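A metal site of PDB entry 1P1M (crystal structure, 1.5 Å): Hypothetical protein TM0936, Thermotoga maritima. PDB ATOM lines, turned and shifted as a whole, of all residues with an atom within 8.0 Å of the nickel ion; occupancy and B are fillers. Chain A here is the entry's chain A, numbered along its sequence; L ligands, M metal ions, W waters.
Water W1 lies within hydrogen-bond range of OD2 of Asp 279 (2.6 Å) and NE2 of His 228 (2.6 Å).
The nickel ion is bound by water W1 (2.1 Å), OD1 of Asp 279 (2.1 Å), NE2 of His 57 (2.1 Å), NE2 of His 55 (2.2 Å), NE2 of His 200 (2.2 Å) and water W2 (2.3 Å).
Within 4 Å of the nickel ion: His 55, His 57, His 200 and Asp 279.
The backbone carbonyl oxygen (O) of Asp 279 lies within hydrogen-bond range of the side-chain hydroxyl (OG1) of Thr 56 (2.9 Å).
The side-chain amide oxygen (OD1) of Asn 250 sits at hydrogen-bond distance from the backbone NH (N) of Asp 279.
The side-chain hydroxyl (OG) of Ser 253 is in hydrogen-bond range of the side-chain carboxylate (OD2) of Asp 279 (2.7 Å).
A ring nitrogen (ND1) of His 57 sits at hydrogen-bond distance from the backbone carbonyl oxygen of Met 114 (2.7 Å).
O of His 55 is in hydrogen-bond range of N of Thr 278, at 3.1 Å.
A ring nitrogen (ND1) of His 200 sits at hydrogen-bond distance from the backbone carbonyl oxygen (O) of His 173.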
ATOM      1  N   HIS A  55     -15.441   4.734  16.615  1.00  0.00           N
ATOM      2  CA  HIS A  55     -15.931   3.440  16.140  1.00  0.00           C
ATOM      3  C   HIS A  55     -16.296   2.466  17.233  1.00  0.00           C
ATOM      4  O   HIS A  55     -15.435   2.031  17.990  1.00  0.00           O
ATOM      5  CB  HIS A  55     -14.938   2.717  15.217  1.00  0.00           C
ATOM      6  CG  HIS A  55     -15.485   1.460  14.601  1.00  0.00           C
ATOM      7  ND1 HIS A  55     -16.538   1.459  13.728  1.00  0.00           N
ATOM      8  CD2 HIS A  55     -15.143   0.152  14.776  1.00  0.00           C
ATOM      9  CE1 HIS A  55     -16.828   0.216  13.378  1.00  0.00           C
ATOM     10  NE2 HIS A  55     -15.997  -0.591  13.998  1.00  0.00           N
ATOM     11  N   THR A  56     -17.569   2.117  17.325  1.00  0.00           N
ATOM     12  CA  THR A  56     -17.997   1.113  18.275  1.00  0.00           C
ATOM     13  C   THR A  56     -19.360   0.549  17.884  1.00  0.00           C
ATOM     14  O   THR A  56     -19.976   0.965  16.895  1.00  0.00           O
ATOM     15  CB  THR A  56     -18.008   1.641  19.735  1.00  0.00           C
ATOM     16  OG1 THR A  56     -18.136   0.538  20.646  1.00  0.00           O
ATOM     17  CG2 THR A  56     -19.150   2.621  19.961  1.00  0.00           C
ATOM     18  N   HIS A  57     -19.795  -0.447  18.646  1.00  0.00           N
ATOM     19  CA  HIS A  57     -21.060  -1.140  18.455  1.00  0.00           C
ATOM     20  C   HIS A  57     -21.472  -1.248  19.920  1.00  0.00           C
ATOM     21  O   HIS A  57     -21.210  -2.250  20.583  1.00  0.00           O
ATOM     22  CB  HIS A  57     -20.792  -2.511  17.833  1.00  0.00           C
ATOM     23  CG  HIS A  57     -19.954  -2.443  16.591  1.00  0.00           C
ATOM     24  ND1 HIS A  57     -20.439  -2.014  15.380  1.00  0.00           N
ATOM     25  CD2 HIS A  57     -18.637  -2.724  16.382  1.00  0.00           C
ATOM     26  CE1 HIS A  57     -19.474  -2.012  14.485  1.00  0.00           C
ATOM     27  NE2 HIS A  57     -18.360  -2.439  15.076  1.00  0.00           N
ATOM     28  N   MET A  60     -22.740  -4.246  22.303  1.00  0.00           N
ATOM     29  CA  MET A  60     -21.873  -5.406  22.382  1.00  0.00           C
ATOM     30  C   MET A  60     -21.209  -5.591  23.740  1.00  0.00           C
ATOM     31  O   MET A  60     -20.518  -6.569  23.965  1.00  0.00           O
ATOM     32  CB  MET A  60     -20.884  -5.399  21.234  1.00  0.00           C
ATOM     33  CG  MET A  60     -21.620  -5.505  19.913  1.00  0.00           C
ATOM     34  SD  MET A  60     -20.660  -6.018  18.505  1.00  0.00           S
ATOM     35  CE  MET A  60     -20.679  -7.860  18.691  1.00  0.00           C
ATOM     36  N   PHE A  72     -11.481 -13.883  12.522  1.00  0.00           N
ATOM     37  CA  PHE A  72     -12.594 -12.986  12.231  1.00  0.00           C
ATOM     38  C   PHE A  72     -13.840 -13.697  11.708  1.00  0.00           C
ATOM     39  O   PHE A  72     -14.942 -13.458  12.207  1.00  0.00           O
ATOM     40  CB  PHE A  72     -12.174 -11.922  11.218  1.00  0.00           C
ATOM     41  CG  PHE A  72     -13.306 -11.043  10.755  1.00  0.00           C
ATOM     42  CD1 PHE A  72     -14.096 -10.346  11.667  1.00  0.00           C
ATOM     43  CD2 PHE A  72     -13.587 -10.914   9.398  1.00  0.00           C
ATOM     44  CE1 PHE A  72     -15.149  -9.536  11.237  1.00  0.00           C
ATOM     45  CE2 PHE A  72     -14.635 -10.106   8.960  1.00  0.00           C
ATOM     46  CZ  PHE A  72     -15.417  -9.408   9.876  1.00  0.00           C
ATOM     47  N   TRP A  75     -15.399 -15.568  14.519  1.00  0.00           N
ATOM     48  CA  TRP A  75     -15.892 -14.600  15.475  1.00  0.00           C
ATOM     49  C   TRP A  75     -17.275 -14.091  15.091  1.00  0.00           C
ATOM     50  O   TRP A  75     -18.221 -14.158  15.877  1.00  0.00           O
ATOM     51  CB  TRP A  75     -14.909 -13.420  15.541  1.00  0.00           C
ATOM     52  CG  TRP A  75     -15.226 -12.355  16.555  1.00  0.00           C
ATOM     53  CD1 TRP A  75     -14.802 -12.298  17.846  1.00  0.00           C
ATOM     54  CD2 TRP A  75     -16.003 -11.163  16.333  1.00  0.00           C
ATOM     55  NE1 TRP A  75     -15.258 -11.140  18.448  1.00  0.00           N
ATOM     56  CE2 TRP A  75     -15.998 -10.439  17.533  1.00  0.00           C
ATOM     57  CE3 TRP A  75     -16.687 -10.650  15.220  1.00  0.00           C
ATOM     58  CZ2 TRP A  75     -16.664  -9.212  17.670  1.00  0.00           C
ATOM     59  CZ3 TRP A  75     -17.353  -9.432  15.361  1.00  0.00           C
ATOM     60  CH2 TRP A  75     -17.330  -8.722  16.577  1.00  0.00           C
ATOM     61  N   MET A 114     -22.378   1.829  15.002  1.00  0.00           N
ATOM     62  CA  MET A 114     -22.853   1.120  13.816  1.00  0.00           C
ATOM     63  C   MET A 114     -23.516  -0.142  14.353  1.00  0.00           C
ATOM     64  O   MET A 114     -22.834  -1.081  14.726  1.00  0.00           O
ATOM     65  CB  MET A 114     -21.704   0.721  12.899  1.00  0.00           C
ATOM     66  CG  MET A 114     -22.152  -0.016  11.643  1.00  0.00           C
ATOM     67  SD  MET A 114     -20.890  -1.013  10.864  1.00  0.00           S
ATOM     68  CE  MET A 114     -19.783   0.293  10.118  1.00  0.00           C
ATOM     69  N   HIS A 173     -21.681  -1.918   6.335  1.00  0.00           N
ATOM     70  CA  HIS A 173     -20.685  -2.693   7.068  1.00  0.00           C
ATOM     71  C   HIS A 173     -19.290  -2.698   6.470  1.00  0.00           C
ATOM     72  O   HIS A 173     -18.297  -2.491   7.195  1.00  0.00           O
ATOM     73  CB  HIS A 173     -21.169  -4.143   7.234  1.00  0.00           C
ATOM     74  CG  HIS A 173     -20.187  -5.012   7.949  1.00  0.00           C
ATOM     75  ND1 HIS A 173     -19.112  -5.600   7.318  1.00  0.00           N
ATOM     76  CD2 HIS A 173     -20.094  -5.353   9.261  1.00  0.00           C
ATOM     77  CE1 HIS A 173     -18.391  -6.268   8.209  1.00  0.00           C
ATOM     78  NE2 HIS A 173     -18.970  -6.132   9.393  1.00  0.00           N
ATOM     79  N   ILE A 199     -17.896   3.058   7.753  1.00  0.00           N
ATOM     80  CA  ILE A 199     -17.773   1.732   7.179  1.00  0.00           C
ATOM     81  C   ILE A 199     -16.471   1.071   7.626  1.00  0.00           C
ATOM     82  O   ILE A 199     -15.522   1.777   7.989  1.00  0.00           O
ATOM     83  CB  ILE A 199     -17.779   1.880   5.627  1.00  0.00           C
ATOM     84  CG1 ILE A 199     -17.655   0.521   4.947  1.00  0.00           C
ATOM     85  CG2 ILE A 199     -16.649   2.818   5.194  1.00  0.00           C
ATOM     86  CD1 ILE A 199     -17.886   0.580   3.440  1.00  0.00           C
ATOM     87  N   HIS A 200     -16.435  -0.253   7.642  1.00  0.00           N
ATOM     88  CA  HIS A 200     -15.221  -0.989   7.998  1.00  0.00           C
ATOM     89  C   HIS A 200     -14.480  -1.075   6.654  1.00  0.00           C
ATOM     90  O   HIS A 200     -14.983  -1.707   5.712  1.00  0.00           O
ATOM     91  CB  HIS A 200     -15.519  -2.408   8.505  1.00  0.00           C
ATOM     92  CG  HIS A 200     -16.280  -2.473   9.799  1.00  0.00           C
ATOM     93  ND1 HIS A 200     -17.519  -3.068   9.897  1.00  0.00           N
ATOM     94  CD2 HIS A 200     -15.932  -2.120  11.055  1.00  0.00           C
ATOM     95  CE1 HIS A 200     -17.903  -3.070  11.168  1.00  0.00           C
ATOM     96  NE2 HIS A 200     -16.957  -2.509  11.886  1.00  0.00           N
ATOM     97  N   GLU A 203     -10.180  -3.866   6.598  1.00  0.00           N
ATOM     98  CA  GLU A 203      -9.860  -4.386   7.923  1.00  0.00           C
ATOM     99  C   GLU A 203      -9.021  -5.663   7.852  1.00  0.00           C
ATOM    100  O   GLU A 203      -8.116  -5.868   8.664  1.00  0.00           O
ATOM    101  CB  GLU A 203     -11.154  -4.679   8.704  1.00  0.00           C
ATOM    102  CG  GLU A 203     -10.914  -5.289  10.080  1.00  0.00           C
ATOM    103  CD  GLU A 203     -12.208  -5.477  10.880  1.00  0.00           C
ATOM    104  OE1 GLU A 203     -13.297  -5.421  10.279  1.00  0.00           O
ATOM    105  OE2 GLU A 203     -12.117  -5.690  12.106  1.00  0.00           O
ATOM    106  N   ALA A 227     -13.339   2.867   9.368  1.00  0.00           N
ATOM    107  CA  ALA A 227     -12.707   2.120  10.421  1.00  0.00           C
ATOM    108  C   ALA A 227     -11.671   1.136   9.911  1.00  0.00           C
ATOM    109  O   ALA A 227     -11.831   0.535   8.842  1.00  0.00           O
ATOM    110  CB  ALA A 227     -13.770   1.371  11.251  1.00  0.00           C
ATOM    111  N   HIS A 228     -10.587   1.029  10.674  1.00  0.00           N
ATOM    112  CA  HIS A 228      -9.475   0.106  10.434  1.00  0.00           C
ATOM    113  C   HIS A 228      -8.422   0.540   9.419  1.00  0.00           C
ATOM    114  O   HIS A 228      -7.337   1.003   9.806  1.00  0.00           O
ATOM    115  CB  HIS A 228     -10.049  -1.268  10.112  1.00  0.00           C
ATOM    116  CG  HIS A 228     -11.018  -1.755  11.145  1.00  0.00           C
ATOM    117  ND1 HIS A 228     -10.695  -1.827  12.478  1.00  0.00           N
ATOM    118  CD2 HIS A 228     -12.309  -2.140  11.048  1.00  0.00           C
ATOM    119  CE1 HIS A 228     -11.747  -2.245  13.162  1.00  0.00           C
ATOM    120  NE2 HIS A 228     -12.742  -2.440  12.312  1.00  0.00           N
ATOM    121  N   ASN A 250      -8.386   1.423  15.109  1.00  0.00           N
ATOM    122  CA  ASN A 250      -8.835   0.521  16.176  1.00  0.00           C
ATOM    123  C   ASN A 250      -7.718  -0.476  16.436  1.00  0.00           C
ATOM    124  O   ASN A 250      -7.844  -1.664  16.093  1.00  0.00           O
ATOM    125  CB  ASN A 250     -10.093  -0.218  15.718  1.00  0.00           C
ATOM    126  CG  ASN A 250     -11.310   0.674  15.660  1.00  0.00           C
ATOM    127  OD1 ASN A 250     -12.277   0.446  16.377  1.00  0.00           O
ATOM    128  ND2 ASN A 250     -11.262   1.686  14.802  1.00  0.00           N
ATOM    129  N   SER A 253      -8.571  -4.017  18.557  1.00  0.00           N
ATOM    130  CA  SER A 253      -9.367  -4.943  17.773  1.00  0.00           C
ATOM    131  C   SER A 253      -8.557  -5.544  16.619  1.00  0.00           C
ATOM    132  O   SER A 253      -8.660  -6.732  16.326  1.00  0.00           O
ATOM    133  CB  SER A 253     -10.609  -4.236  17.221  1.00  0.00           C
ATOM    134  OG  SER A 253     -11.393  -5.128  16.442  1.00  0.00           O
ATOM    135  N   LEU A 257      -8.077  -9.696  16.660  1.00  0.00           N
ATOM    136  CA  LEU A 257      -8.639 -10.528  15.606  1.00  0.00           C
ATOM    137  C   LEU A 257      -7.612 -10.957  14.552  1.00  0.00           C
ATOM    138  O   LEU A 257      -7.968 -11.475  13.500  1.00  0.00           O
ATOM    139  CB  LEU A 257      -9.807  -9.803  14.931  1.00  0.00           C
ATOM    140  CG  LEU A 257     -11.038  -9.572  15.819  1.00  0.00           C
ATOM    141  CD1 LEU A 257     -12.081  -8.771  15.050  1.00  0.00           C
ATOM    142  CD2 LEU A 257     -11.609 -10.910  16.267  1.00  0.00           C
ATOM    143  N   THR A 278     -12.615   2.197  19.339  1.00  0.00           N
ATOM    144  CA  THR A 278     -12.410   1.014  20.173  1.00  0.00           C
ATOM    145  C   THR A 278     -12.947  -0.277  19.551  1.00  0.00           C
ATOM    146  O   THR A 278     -12.465  -1.365  19.849  1.00  0.00           O
ATOM    147  CB  THR A 278     -13.144   1.157  21.522  1.00  0.00           C
ATOM    148  OG1 THR A 278     -14.535   1.361  21.264  1.00  0.00           O
ATOM    149  CG2 THR A 278     -12.610   2.341  22.304  1.00  0.00           C
ATOM    150  N   ASP A 279     -13.957  -0.126  18.703  1.00  0.00           N
ATOM    151  CA  ASP A 279     -14.704  -1.216  18.093  1.00  0.00           C
ATOM    152  C   ASP A 279     -15.605  -1.695  19.243  1.00  0.00           C
ATOM    153  O   ASP A 279     -15.759  -0.989  20.233  1.00  0.00           O
ATOM    154  CB  ASP A 279     -13.804  -2.354  17.568  1.00  0.00           C
ATOM    155  CG  ASP A 279     -14.368  -2.995  16.295  1.00  0.00           C
ATOM    156  OD1 ASP A 279     -15.495  -2.632  15.891  1.00  0.00           O
ATOM    157  OD2 ASP A 279     -13.689  -3.843  15.683  1.00  0.00           O
ATOM    158  N   GLY A 280     -16.217  -2.867  19.100  1.00  0.00           N
ATOM    159  CA  GLY A 280     -17.096  -3.369  20.139  1.00  0.00           C
ATOM    160  C   GLY A 280     -16.396  -4.132  21.248  1.00  0.00           C
ATOM    161  O   GLY A 280     -15.280  -4.608  21.065  1.00  0.00           O
ATOM    162  N   SER A 283     -14.532  -7.630  20.742  1.00  0.00           N
ATOM    163  CA  SER A 283     -13.249  -7.763  20.060  1.00  0.00           C
ATOM    164  C   SER A 283     -12.292  -6.641  20.459  1.00  0.00           C
ATOM    165  O   SER A 283     -11.668  -5.979  19.628  1.00  0.00           O
ATOM    166  CB  SER A 283     -13.408  -7.819  18.529  1.00  0.00           C
ATOM    167  OG  SER A 283     -13.729  -6.572  17.968  1.00  0.00           O
HETATM  168  N1  LIG L   1     -25.303  -8.134  11.509  1.00  0.00           N
HETATM  169  C1  LIG L   1     -26.090  -6.875  11.399  1.00  0.00           C
HETATM  170  C2  LIG L   1     -27.476  -7.154  10.838  1.00  0.00           C
HETATM  171  O1  LIG L   1     -28.272  -6.198  10.756  1.00  0.00           O
HETATM  172  C3  LIG L   1     -25.375  -5.874  10.487  1.00  0.00           C
HETATM  173  C4  LIG L   1     -24.114  -5.273  11.084  1.00  0.00           C
HETATM  174  S1  LIG L   1     -24.469  -4.268  12.534  1.00  0.00           S
HETATM  175  C5  LIG L   1     -22.800  -3.729  12.956  1.00  0.00           C
HETATM  176  O2  LIG L   1     -27.737  -8.329  10.489  1.00  0.00           O
HETATM  177 NI    NI M   1     -16.525  -2.704  14.060  1.00  0.00          NI
HETATM  178  O   HOH W   1     -14.829  -3.673  13.350  1.00  0.00           O
HETATM  179  O   HOH W   2     -17.027  -4.905  14.483  1.00  0.00           O
